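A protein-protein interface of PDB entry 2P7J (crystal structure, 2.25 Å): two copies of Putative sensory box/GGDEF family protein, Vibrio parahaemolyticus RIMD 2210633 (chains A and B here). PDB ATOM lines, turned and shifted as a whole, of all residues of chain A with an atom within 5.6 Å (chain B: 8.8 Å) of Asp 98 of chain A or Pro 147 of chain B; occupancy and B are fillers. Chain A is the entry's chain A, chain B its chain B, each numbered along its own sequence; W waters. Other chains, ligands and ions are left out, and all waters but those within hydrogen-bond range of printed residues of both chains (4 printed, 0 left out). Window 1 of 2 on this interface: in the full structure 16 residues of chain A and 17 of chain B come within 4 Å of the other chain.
O of Lys 100 of chain A lies close to OE2 of Glu 206 of chain B (3.0 Å).
N of Asp 98 of chain A lies within hydrogen-bond range of O of Ile 103 of chain A (3.0 Å).
OE2 of Glu 206 of chain B is in salt-bridge range of NH2 of Arg 217 of chain B, 2.7 Å away.
The backbone NH (N) of Ile 103 of chain A sits close to the side-chain hydroxyl (OG1) of Thr 101 of chain A.
O of Pro 147 of chain B sits at hydrogen-bond distance from OG of Ser 149 of chain B (3.2 Å).
The side-chain hydroxyl (OG1) of Thr 101 of chain A lies within hydrogen-bond range of the side-chain carboxylate (OD2) of Asp 98 of chain A (2.6 Å).
Among the printed residues, pairs that only touch across the chains: Lys 96 of chain A with Tyr 146 of chain B (3.7 Å), Asp 98 of chain A with Tyr 146 of chain B (3.4 Å), Asp 98 of chain A with Pro 147 of chain B (3.8 Å), Thr 101 of chain A with Leu 148 of chain B (3.7 Å), Thr 101 of chain A with Glu 206 of chain B (3.3 Å), Thr 101 of chain A with Arg 217 of chain B (3.97 Å), Ile 103 of chain A with Tyr 146 of chain B (3.5 Å), Ile 103 of chain A with Ile 214 of chain B (3.7 Å) and Pro 147 of chain A with Asp 98 of chain B (3.9 Å).
Asp 98 of chain A touches just these residues of chain B: Tyr 146 (3.4 Å) and Pro 147 (3.8 Å).
Of the printed residues of chain A, Pro 147 of chain B touches Asp 98 (3.8 Å).
No residue of chain B comes within 4 Å of Tyr 97 of chain A.
Printed residues of chain B within 4 Å of Ile 103 of chain A: Tyr 146 and Ile 214.
Printed residues of chain B within 4 Å of Lys 100 of chain A: Glu 206.
Of the printed residues of chain A, Tyr 146 of chain B touches Lys 96, Asp 98 and Ile 103.
Of the printed residues of chain B, Thr 101 of chain A touches Leu 148 (3.7 Å), Glu 206 (3.3 Å) and Arg 217 (3.97 Å).
Pro 150 of chain B touches none of the printed residues of chain A.
Of the 19 printed residues of chain B, 7 touch a printed residue of chain A.
Hydrophobic or aromatic side chains of chain B that line the printed part of chain A: Tyr 146, Leu 148 and Ile 214.
Printed residues of chain A that touch a printed residue of chain B: Lys 96, Asp 98, Lys 100, Thr 101, Ile 103 and Pro 147.
Hydrophobic or aromatic side chains of chain A that line the printed part of chain B: Ile 103.
Along chain A the printed residues that touch a printed residue of chain B span positions 96 to 147.
Among the printed residues, 10 pairs touch across the chains.
Among the printed residues, no Asp or Glu carboxylate lies within 4 Å of a Lys or Arg side-chain nitrogen of the other chain.
Asp 98 of chain A touches Pro 147 of chain B, and with the chains exchanged Pro 147 of chain A touches Asp 98 of chain B.
4 positions are printed for both chains.
Of the 10 pairs that touch across the chains among the printed residues, 2 have their exchanged pair printed and touching as well.
Water W4 lies within hydrogen-bond range of the side-chain amino group (NZ) of Lys 96 of chain A (2.6 Å) and the backbone NH (N) of Tyr 146 of chain B (2.8 Å).
Water W1 bridges the side-chain carboxylate of Glu 216 of chain B (2.6 Å) and the backbone carbonyl oxygen of Thr 101 of chain A (2.9 Å).
Water W3 lies within hydrogen-bond range of OD2 of Asp 98 of chain A (2.7 Å) and N of Leu 148 of chain B (2.9 Å).
Water W2 bridges the guanidinium group of Arg 217 of chain B (2.9 Å) and the backbone carbonyl oxygen of Thr 101 of chain A (3.0 Å).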
ATOM      1  N   LYS A  80     -16.439 -20.107 -21.661  1.00  0.00           N
ATOM      2  CA  LYS A  80     -17.544 -20.734 -22.306  1.00  0.00           C
ATOM      3  C   LYS A  80     -17.106 -21.630 -23.459  1.00  0.00           C
ATOM      4  O   LYS A  80     -17.898 -22.428 -23.936  1.00  0.00           O
ATOM      5  CB  LYS A  80     -18.583 -19.732 -22.720  1.00  0.00           C
ATOM      6  CG  LYS A  80     -18.144 -18.648 -23.627  1.00  0.00           C
ATOM      7  CD  LYS A  80     -19.417 -17.878 -24.048  1.00  0.00           C
ATOM      8  CE  LYS A  80     -20.613 -18.826 -24.116  1.00  0.00           C
ATOM      9  NZ  LYS A  80     -21.212 -18.846 -25.494  1.00  0.00           N
ATOM     10  N   LYS A  96     -17.435 -26.848 -25.254  1.00  0.00           N
ATOM     11  CA  LYS A  96     -18.372 -25.807 -24.843  1.00  0.00           C
ATOM     12  C   LYS A  96     -18.748 -26.001 -23.375  1.00  0.00           C
ATOM     13  O   LYS A  96     -18.876 -27.140 -22.900  1.00  0.00           O
ATOM     14  CB  LYS A  96     -19.648 -25.827 -25.706  1.00  0.00           C
ATOM     15  CG  LYS A  96     -19.434 -25.475 -27.163  1.00  0.00           C
ATOM     16  CD  LYS A  96     -20.574 -26.024 -28.021  1.00  0.00           C
ATOM     17  CE  LYS A  96     -21.752 -25.071 -28.065  1.00  0.00           C
ATOM     18  NZ  LYS A  96     -22.831 -25.498 -27.105  1.00  0.00           N
ATOM     19  N   TYR A  97     -18.951 -24.887 -22.674  1.00  0.00           N
ATOM     20  CA  TYR A  97     -19.440 -24.910 -21.282  1.00  0.00           C
ATOM     21  C   TYR A  97     -20.610 -23.948 -21.125  1.00  0.00           C
ATOM     22  O   TYR A  97     -20.607 -22.836 -21.663  1.00  0.00           O
ATOM     23  CB  TYR A  97     -18.319 -24.552 -20.300  1.00  0.00           C
ATOM     24  CG  TYR A  97     -18.734 -24.420 -18.840  1.00  0.00           C
ATOM     25  CD1 TYR A  97     -18.912 -25.559 -18.036  1.00  0.00           C
ATOM     26  CD2 TYR A  97     -18.922 -23.158 -18.252  1.00  0.00           C
ATOM     27  CE1 TYR A  97     -19.279 -25.451 -16.682  1.00  0.00           C
ATOM     28  CE2 TYR A  97     -19.296 -23.037 -16.887  1.00  0.00           C
ATOM     29  CZ  TYR A  97     -19.457 -24.193 -16.110  1.00  0.00           C
ATOM     30  OH  TYR A  97     -19.832 -24.098 -14.766  1.00  0.00           O
ATOM     31  N   ASP A  98     -21.614 -24.400 -20.394  1.00  0.00           N
ATOM     32  CA  ASP A  98     -22.823 -23.616 -20.138  1.00  0.00           C
ATOM     33  C   ASP A  98     -22.954 -23.433 -18.612  1.00  0.00           C
ATOM     34  O   ASP A  98     -23.244 -24.388 -17.889  1.00  0.00           O
ATOM     35  CB  ASP A  98     -24.049 -24.346 -20.708  1.00  0.00           C
ATOM     36  CG  ASP A  98     -25.372 -23.634 -20.382  1.00  0.00           C
ATOM     37  OD1 ASP A  98     -25.517 -22.464 -20.749  1.00  0.00           O
ATOM     38  OD2 ASP A  98     -26.259 -24.253 -19.769  1.00  0.00           O
ATOM     39  N   PHE A  99     -22.708 -22.219 -18.130  1.00  0.00           N
ATOM     40  CA  PHE A  99     -22.573 -22.025 -16.681  1.00  0.00           C
ATOM     41  C   PHE A  99     -23.872 -22.206 -15.905  1.00  0.00           C
ATOM     42  O   PHE A  99     -23.823 -22.549 -14.705  1.00  0.00           O
ATOM     43  CB  PHE A  99     -21.908 -20.688 -16.319  1.00  0.00           C
ATOM     44  CG  PHE A  99     -22.793 -19.500 -16.468  1.00  0.00           C
ATOM     45  CD1 PHE A  99     -23.687 -19.143 -15.445  1.00  0.00           C
ATOM     46  CD2 PHE A  99     -22.692 -18.694 -17.594  1.00  0.00           C
ATOM     47  CE1 PHE A  99     -24.518 -18.002 -15.578  1.00  0.00           C
ATOM     48  CE2 PHE A  99     -23.512 -17.547 -17.753  1.00  0.00           C
ATOM     49  CZ  PHE A  99     -24.435 -17.205 -16.738  1.00  0.00           C
ATOM     50  N   LYS A 100     -25.006 -21.975 -16.586  1.00  0.00           N
ATOM     51  CA  LYS A 100     -26.340 -22.099 -15.955  1.00  0.00           C
ATOM     52  C   LYS A 100     -26.654 -23.533 -15.547  1.00  0.00           C
ATOM     53  O   LYS A 100     -27.132 -23.770 -14.440  1.00  0.00           O
ATOM     54  CB  LYS A 100     -27.434 -21.491 -16.837  1.00  0.00           C
ATOM     55  CG  LYS A 100     -27.770 -20.062 -16.389  1.00  0.00           C
ATOM     56  CD  LYS A 100     -28.071 -19.093 -17.559  1.00  0.00           C
ATOM     57  CE  LYS A 100     -28.606 -17.719 -17.037  1.00  0.00           C
ATOM     58  NZ  LYS A 100     -27.905 -17.215 -15.805  1.00  0.00           N
ATOM     59  N   THR A 101     -26.305 -24.488 -16.409  1.00  0.00           N
ATOM     60  CA  THR A 101     -26.421 -25.913 -16.098  1.00  0.00           C
ATOM     61  C   THR A 101     -25.159 -26.559 -15.504  1.00  0.00           C
ATOM     62  O   THR A 101     -25.236 -27.630 -14.901  1.00  0.00           O
ATOM     63  CB  THR A 101     -26.737 -26.701 -17.383  1.00  0.00           C
ATOM     64  OG1 THR A 101     -25.743 -26.395 -18.352  1.00  0.00           O
ATOM     65  CG2 THR A 101     -28.095 -26.304 -17.950  1.00  0.00           C
ATOM     66  N   SER A 102     -23.990 -25.953 -15.725  1.00  0.00           N
ATOM     67  CA  SER A 102     -22.738 -26.579 -15.322  1.00  0.00           C
ATOM     68  C   SER A 102     -22.268 -27.660 -16.294  1.00  0.00           C
ATOM     69  O   SER A 102     -21.323 -28.391 -16.013  1.00  0.00           O
ATOM     70  N   ILE A 103     -22.909 -27.757 -17.451  1.00  0.00           N
ATOM     71  CA  ILE A 103     -22.556 -28.803 -18.426  1.00  0.00           C
ATOM     72  C   ILE A 103     -21.457 -28.383 -19.395  1.00  0.00           C
ATOM     73  O   ILE A 103     -21.586 -27.374 -20.068  1.00  0.00           O
ATOM     74  CB  ILE A 103     -23.787 -29.317 -19.213  1.00  0.00           C
ATOM     75  CG1 ILE A 103     -24.749 -30.034 -18.247  1.00  0.00           C
ATOM     76  CG2 ILE A 103     -23.345 -30.308 -20.299  1.00  0.00           C
ATOM     77  CD1 ILE A 103     -26.224 -30.004 -18.687  1.00  0.00           C
ATOM     78  N   ALA A 104     -20.386 -29.180 -19.420  1.00  0.00           N
ATOM     79  CA  ALA A 104     -19.260 -29.044 -20.350  1.00  0.00           C
ATOM     80  C   ALA A 104     -19.160 -30.270 -21.232  1.00  0.00           C
ATOM     81  O   ALA A 104     -19.417 -31.388 -20.780  1.00  0.00           O
ATOM     82  CB  ALA A 104     -17.942 -28.875 -19.570  1.00  0.00           C
ATOM     83  N   PRO A 147     -28.286 -15.998 -27.476  1.00  0.00           N
ATOM     84  CA  PRO A 147     -28.148 -14.667 -26.832  1.00  0.00           C
ATOM     85  C   PRO A 147     -26.739 -14.126 -27.010  1.00  0.00           C
ATOM     86  O   PRO A 147     -25.760 -14.887 -26.966  1.00  0.00           O
ATOM     87  CB  PRO A 147     -28.404 -14.939 -25.338  1.00  0.00           C
ATOM     88  CG  PRO A 147     -29.074 -16.300 -25.283  1.00  0.00           C
ATOM     89  CD  PRO A 147     -28.705 -17.054 -26.531  1.00  0.00           C
ATOM     90  N   LYS B  80     -38.853 -18.353 -31.659  1.00  0.00           N
ATOM     91  CA  LYS B  80     -37.424 -18.113 -31.789  1.00  0.00           C
ATOM     92  C   LYS B  80     -36.838 -18.515 -33.128  1.00  0.00           C
ATOM     93  O   LYS B  80     -35.768 -18.061 -33.462  1.00  0.00           O
ATOM     94  CB  LYS B  80     -36.630 -18.682 -30.613  1.00  0.00           C
ATOM     95  CG  LYS B  80     -36.797 -20.104 -30.358  1.00  0.00           C
ATOM     96  CD  LYS B  80     -35.790 -20.484 -29.282  1.00  0.00           C
ATOM     97  CE  LYS B  80     -34.422 -19.912 -29.601  1.00  0.00           C
ATOM     98  NZ  LYS B  80     -33.421 -20.371 -28.628  1.00  0.00           N
ATOM     99  N   ASP B  98     -34.459 -13.220 -31.273  1.00  0.00           N
ATOM    100  CA  ASP B  98     -33.950 -13.234 -29.910  1.00  0.00           C
ATOM    101  C   ASP B  98     -34.794 -12.275 -29.056  1.00  0.00           C
ATOM    102  O   ASP B  98     -34.732 -11.052 -29.223  1.00  0.00           O
ATOM    103  CB  ASP B  98     -32.464 -12.852 -29.906  1.00  0.00           C
ATOM    104  CG  ASP B  98     -31.903 -12.689 -28.518  1.00  0.00           C
ATOM    105  OD1 ASP B  98     -31.794 -13.683 -27.774  1.00  0.00           O
ATOM    106  OD2 ASP B  98     -31.538 -11.556 -28.175  1.00  0.00           O
ATOM    107  N   LYS B 100     -34.700 -11.291 -25.876  1.00  0.00           N
ATOM    108  CA  LYS B 100     -33.990 -10.337 -25.000  1.00  0.00           C
ATOM    109  C   LYS B 100     -33.687  -9.034 -25.727  1.00  0.00           C
ATOM    110  O   LYS B 100     -33.967  -7.951 -25.210  1.00  0.00           O
ATOM    111  CB  LYS B 100     -32.688 -10.929 -24.429  1.00  0.00           C
ATOM    112  CG  LYS B 100     -32.873 -12.062 -23.373  1.00  0.00           C
ATOM    113  CD  LYS B 100     -33.289 -11.489 -21.978  1.00  0.00           C
ATOM    114  CE  LYS B 100     -33.623 -12.583 -20.968  1.00  0.00           C
ATOM    115  NZ  LYS B 100     -32.546 -13.616 -20.893  1.00  0.00           N
ATOM    116  N   LEU B 137     -35.968 -30.106 -26.664  1.00  0.00           N
ATOM    117  CA  LEU B 137     -34.794 -29.218 -26.732  1.00  0.00           C
ATOM    118  C   LEU B 137     -34.242 -29.008 -28.152  1.00  0.00           C
ATOM    119  O   LEU B 137     -34.171 -29.946 -28.969  1.00  0.00           O
ATOM    120  CB  LEU B 137     -33.699 -29.703 -25.782  1.00  0.00           C
ATOM    121  CG  LEU B 137     -34.080 -29.748 -24.298  1.00  0.00           C
ATOM    122  CD1 LEU B 137     -32.959 -30.431 -23.465  1.00  0.00           C
ATOM    123  CD2 LEU B 137     -34.456 -28.335 -23.745  1.00  0.00           C
ATOM    124  N   GLU B 138     -33.876 -27.765 -28.461  1.00  0.00           N
ATOM    125  CA  GLU B 138     -33.278 -27.482 -29.759  1.00  0.00           C
ATOM    126  C   GLU B 138     -31.865 -28.069 -29.887  1.00  0.00           C
ATOM    127  O   GLU B 138     -31.138 -28.203 -28.899  1.00  0.00           O
ATOM    128  CB  GLU B 138     -33.237 -25.987 -30.019  1.00  0.00           C
ATOM    129  CG  GLU B 138     -34.547 -25.424 -30.469  1.00  0.00           C
ATOM    130  CD  GLU B 138     -34.493 -23.942 -30.628  1.00  0.00           C
ATOM    131  OE1 GLU B 138     -33.421 -23.358 -30.327  1.00  0.00           O
ATOM    132  OE2 GLU B 138     -35.512 -23.357 -31.062  1.00  0.00           O
ATOM    133  N   ARG B 139     -31.502 -28.403 -31.125  1.00  0.00           N
ATOM    134  CA  ARG B 139     -30.226 -29.017 -31.457  1.00  0.00           C
ATOM    135  C   ARG B 139     -29.663 -28.422 -32.746  1.00  0.00           C
ATOM    136  O   ARG B 139     -30.433 -27.917 -33.590  1.00  0.00           O
ATOM    137  CB  ARG B 139     -30.405 -30.519 -31.644  1.00  0.00           C
ATOM    138  CG  ARG B 139     -30.656 -31.269 -30.353  1.00  0.00           C
ATOM    139  CD  ARG B 139     -30.951 -32.758 -30.583  1.00  0.00           C
ATOM    140  NE  ARG B 139     -31.330 -33.344 -29.308  1.00  0.00           N
ATOM    141  CZ  ARG B 139     -30.488 -33.941 -28.460  1.00  0.00           C
ATOM    142  NH1 ARG B 139     -29.181 -34.095 -28.768  1.00  0.00           N
ATOM    143  NH2 ARG B 139     -30.964 -34.401 -27.301  1.00  0.00           N
ATOM    144  N   LEU B 144     -27.048 -30.547 -28.594  1.00  0.00           N
ATOM    145  CA  LEU B 144     -27.898 -29.638 -27.858  1.00  0.00           C
ATOM    146  C   LEU B 144     -27.405 -28.215 -27.977  1.00  0.00           C
ATOM    147  O   LEU B 144     -26.202 -27.946 -27.887  1.00  0.00           O
ATOM    148  CB  LEU B 144     -27.940 -30.064 -26.382  1.00  0.00           C
ATOM    149  CG  LEU B 144     -28.802 -31.269 -26.035  1.00  0.00           C
ATOM    150  CD1 LEU B 144     -28.544 -31.686 -24.605  1.00  0.00           C
ATOM    151  CD2 LEU B 144     -30.278 -30.899 -26.224  1.00  0.00           C
ATOM    152  N   VAL B 145     -28.343 -27.299 -28.180  1.00  0.00           N
ATOM    153  CA  VAL B 145     -28.033 -25.883 -28.165  1.00  0.00           C
ATOM    154  C   VAL B 145     -28.037 -25.418 -26.704  1.00  0.00           C
ATOM    155  O   VAL B 145     -28.874 -25.854 -25.927  1.00  0.00           O
ATOM    156  CB  VAL B 145     -29.052 -25.071 -28.994  1.00  0.00           C
ATOM    157  CG1 VAL B 145     -28.790 -23.569 -28.849  1.00  0.00           C
ATOM    158  CG2 VAL B 145     -29.008 -25.475 -30.469  1.00  0.00           C
ATOM    159  N   TYR B 146     -27.073 -24.567 -26.349  1.00  0.00           N
ATOM    160  CA  TYR B 146     -26.937 -23.975 -25.026  1.00  0.00           C
ATOM    161  C   TYR B 146     -26.864 -22.465 -25.194  1.00  0.00           C
ATOM    162  O   TYR B 146     -26.219 -21.982 -26.135  1.00  0.00           O
ATOM    163  CB  TYR B 146     -25.664 -24.441 -24.336  1.00  0.00           C
ATOM    164  CG  TYR B 146     -25.717 -25.872 -23.880  1.00  0.00           C
ATOM    165  CD1 TYR B 146     -26.206 -26.214 -22.617  1.00  0.00           C
ATOM    166  CD2 TYR B 146     -25.286 -26.900 -24.717  1.00  0.00           C
ATOM    167  CE1 TYR B 146     -26.249 -27.551 -22.201  1.00  0.00           C
ATOM    168  CE2 TYR B 146     -25.338 -28.227 -24.318  1.00  0.00           C
ATOM    169  CZ  TYR B 146     -25.822 -28.543 -23.067  1.00  0.00           C
ATOM    170  OH  TYR B 146     -25.849 -29.870 -22.685  1.00  0.00           O
ATOM    171  N   PRO B 147     -27.525 -21.711 -24.281  1.00  0.00           N
ATOM    172  CA  PRO B 147     -28.370 -22.240 -23.184  1.00  0.00           C
ATOM    173  C   PRO B 147     -29.470 -23.169 -23.701  1.00  0.00           C
ATOM    174  O   PRO B 147     -29.909 -23.024 -24.839  1.00  0.00           O
ATOM    175  CB  PRO B 147     -28.983 -20.985 -22.577  1.00  0.00           C
ATOM    176  CG  PRO B 147     -27.988 -19.907 -22.886  1.00  0.00           C
ATOM    177  CD  PRO B 147     -27.432 -20.238 -24.244  1.00  0.00           C
ATOM    178  N   LEU B 148     -29.902 -24.106 -22.866  1.00  0.00           N
ATOM    179  CA  LEU B 148     -30.922 -25.086 -23.264  1.00  0.00           C
ATOM    180  C   LEU B 148     -32.245 -24.426 -23.695  1.00  0.00           C
ATOM    181  O   LEU B 148     -32.737 -23.539 -23.002  1.00  0.00           O
ATOM    182  CB  LEU B 148     -31.138 -26.100 -22.148  1.00  0.00           C
ATOM    183  CG  LEU B 148     -29.908 -26.987 -21.874  1.00  0.00           C
ATOM    184  CD1 LEU B 148     -30.091 -27.896 -20.678  1.00  0.00           C
ATOM    185  CD2 LEU B 148     -29.558 -27.812 -23.101  1.00  0.00           C
ATOM    186  N   SER B 149     -32.777 -24.827 -24.859  1.00  0.00           N
ATOM    187  CA  SER B 149     -33.990 -24.200 -25.413  1.00  0.00           C
ATOM    188  C   SER B 149     -35.118 -25.173 -25.688  1.00  0.00           C
ATOM    189  O   SER B 149     -35.184 -25.752 -26.785  1.00  0.00           O
ATOM    190  CB  SER B 149     -33.697 -23.478 -26.739  1.00  0.00           C
ATOM    191  OG  SER B 149     -32.520 -22.708 -26.660  1.00  0.00           O
ATOM    192  N   PRO B 150     -36.022 -25.352 -24.713  1.00  0.00           N
ATOM    193  CA  PRO B 150     -37.184 -26.195 -25.018  1.00  0.00           C
ATOM    194  C   PRO B 150     -38.076 -25.477 -26.033  1.00  0.00           C
ATOM    195  O   PRO B 150     -38.366 -24.277 -25.887  1.00  0.00           O
ATOM    196  CB  PRO B 150     -37.881 -26.356 -23.673  1.00  0.00           C
ATOM    197  CG  PRO B 150     -37.429 -25.135 -22.848  1.00  0.00           C
ATOM    198  CD  PRO B 150     -36.044 -24.804 -23.342  1.00  0.00           C
ATOM    199  N   GLU B 175     -39.285 -21.591 -22.961  1.00  0.00           N
ATOM    200  CA  GLU B 175     -38.747 -20.697 -21.940  1.00  0.00           C
ATOM    201  C   GLU B 175     -39.367 -19.302 -21.913  1.00  0.00           C
ATOM    202  O   GLU B 175     -39.816 -18.841 -20.863  1.00  0.00           O
ATOM    203  CB  GLU B 175     -37.223 -20.589 -21.974  1.00  0.00           C
ATOM    204  CG  GLU B 175     -36.774 -20.285 -20.567  1.00  0.00           C
ATOM    205  CD  GLU B 175     -35.512 -20.950 -20.231  1.00  0.00           C
ATOM    206  OE1 GLU B 175     -34.484 -20.539 -20.837  1.00  0.00           O
ATOM    207  OE2 GLU B 175     -35.555 -21.857 -19.363  1.00  0.00           O
ATOM    208  N   GLU B 206     -34.151 -24.263 -12.267  1.00  0.00           N
ATOM    209  CA  GLU B 206     -33.489 -24.742 -13.467  1.00  0.00           C
ATOM    210  C   GLU B 206     -32.856 -26.113 -13.319  1.00  0.00           C
ATOM    211  O   GLU B 206     -32.741 -26.876 -14.299  1.00  0.00           O
ATOM    212  CB  GLU B 206     -32.455 -23.704 -13.945  1.00  0.00           C
ATOM    213  CG  GLU B 206     -31.349 -24.239 -14.902  1.00  0.00           C
ATOM    214  CD  GLU B 206     -30.141 -24.874 -14.158  1.00  0.00           C
ATOM    215  OE1 GLU B 206     -29.895 -24.536 -12.976  1.00  0.00           O
ATOM    216  OE2 GLU B 206     -29.433 -25.703 -14.758  1.00  0.00           O
ATOM    217  N   TYR B 210     -35.591 -31.151 -17.601  1.00  0.00           N
ATOM    218  CA  TYR B 210     -35.124 -32.004 -18.683  1.00  0.00           C
ATOM    219  C   TYR B 210     -34.448 -33.320 -18.251  1.00  0.00           C
ATOM    220  O   TYR B 210     -33.548 -33.836 -18.929  1.00  0.00           O
ATOM    221  CB  TYR B 210     -34.237 -31.210 -19.669  1.00  0.00           C
ATOM    222  CG  TYR B 210     -34.556 -29.715 -19.802  1.00  0.00           C
ATOM    223  CD1 TYR B 210     -35.826 -29.263 -20.190  1.00  0.00           C
ATOM    224  CD2 TYR B 210     -33.571 -28.760 -19.566  1.00  0.00           C
ATOM    225  CE1 TYR B 210     -36.094 -27.891 -20.315  1.00  0.00           C
ATOM    226  CE2 TYR B 210     -33.833 -27.387 -19.686  1.00  0.00           C
ATOM    227  CZ  TYR B 210     -35.093 -26.966 -20.068  1.00  0.00           C
ATOM    228  OH  TYR B 210     -35.334 -25.607 -20.190  1.00  0.00           O
ATOM    229  N   ILE B 214     -31.012 -34.822 -19.885  1.00  0.00           N
ATOM    230  CA  ILE B 214     -29.793 -34.624 -19.093  1.00  0.00           C
ATOM    231  C   ILE B 214     -29.743 -35.735 -18.021  1.00  0.00           C
ATOM    232  O   ILE B 214     -30.618 -35.785 -17.153  1.00  0.00           O
ATOM    233  CB  ILE B 214     -29.728 -33.190 -18.418  1.00  0.00           C
ATOM    234  CG1 ILE B 214     -30.143 -32.041 -19.363  1.00  0.00           C
ATOM    235  CG2 ILE B 214     -28.359 -32.922 -17.804  1.00  0.00           C
ATOM    236  CD1 ILE B 214     -29.534 -32.055 -20.783  1.00  0.00           C
ATOM    237  N   GLU B 216     -27.910 -36.759 -15.394  1.00  0.00           N
ATOM    238  CA  GLU B 216     -27.726 -36.362 -14.004  1.00  0.00           C
ATOM    239  C   GLU B 216     -29.039 -35.956 -13.302  1.00  0.00           C
ATOM    240  O   GLU B 216     -29.056 -35.719 -12.092  1.00  0.00           O
ATOM    241  CB  GLU B 216     -26.727 -35.191 -13.984  1.00  0.00           C
ATOM    242  CG  GLU B 216     -27.018 -34.163 -15.086  1.00  0.00           C
ATOM    243  CD  GLU B 216     -25.842 -33.269 -15.471  1.00  0.00           C
ATOM    244  OE1 GLU B 216     -25.669 -32.207 -14.833  1.00  0.00           O
ATOM    245  OE2 GLU B 216     -25.131 -33.598 -16.453  1.00  0.00           O
ATOM    246  N   ARG B 217     -30.131 -35.884 -14.065  1.00  0.00           N
ATOM    247  CA  ARG B 217     -31.413 -35.334 -13.582  1.00  0.00           C
ATOM    248  C   ARG B 217     -32.590 -36.306 -13.744  1.00  0.00           C
ATOM    249  O   ARG B 217     -33.750 -35.924 -13.587  1.00  0.00           O
ATOM    250  CB  ARG B 217     -31.727 -34.030 -14.324  1.00  0.00           C
ATOM    251  CG  ARG B 217     -30.840 -32.848 -14.003  1.00  0.00           C
ATOM    252  CD  ARG B 217     -30.954 -31.803 -15.106  1.00  0.00           C
ATOM    253  NE  ARG B 217     -30.199 -30.586 -14.798  1.00  0.00           N
ATOM    254  CZ  ARG B 217     -30.434 -29.378 -15.310  1.00  0.00           C
ATOM    255  NH1 ARG B 217     -31.417 -29.175 -16.182  1.00  0.00           N
ATOM    256  NH2 ARG B 217     -29.673 -28.362 -14.944  1.00  0.00           N
HETATM  257  O   HOH W   1     -23.955 -30.236 -14.434  1.00  0.00           O
HETATM  258  O   HOH W   2     -27.504 -28.071 -13.033  1.00  0.00           O
HETATM  259  O   HOH W   3     -28.862 -23.684 -20.146  1.00  0.00           O
HETATM  260  O   HOH W   4     -24.901 -24.384 -28.181  1.00  0.00           O
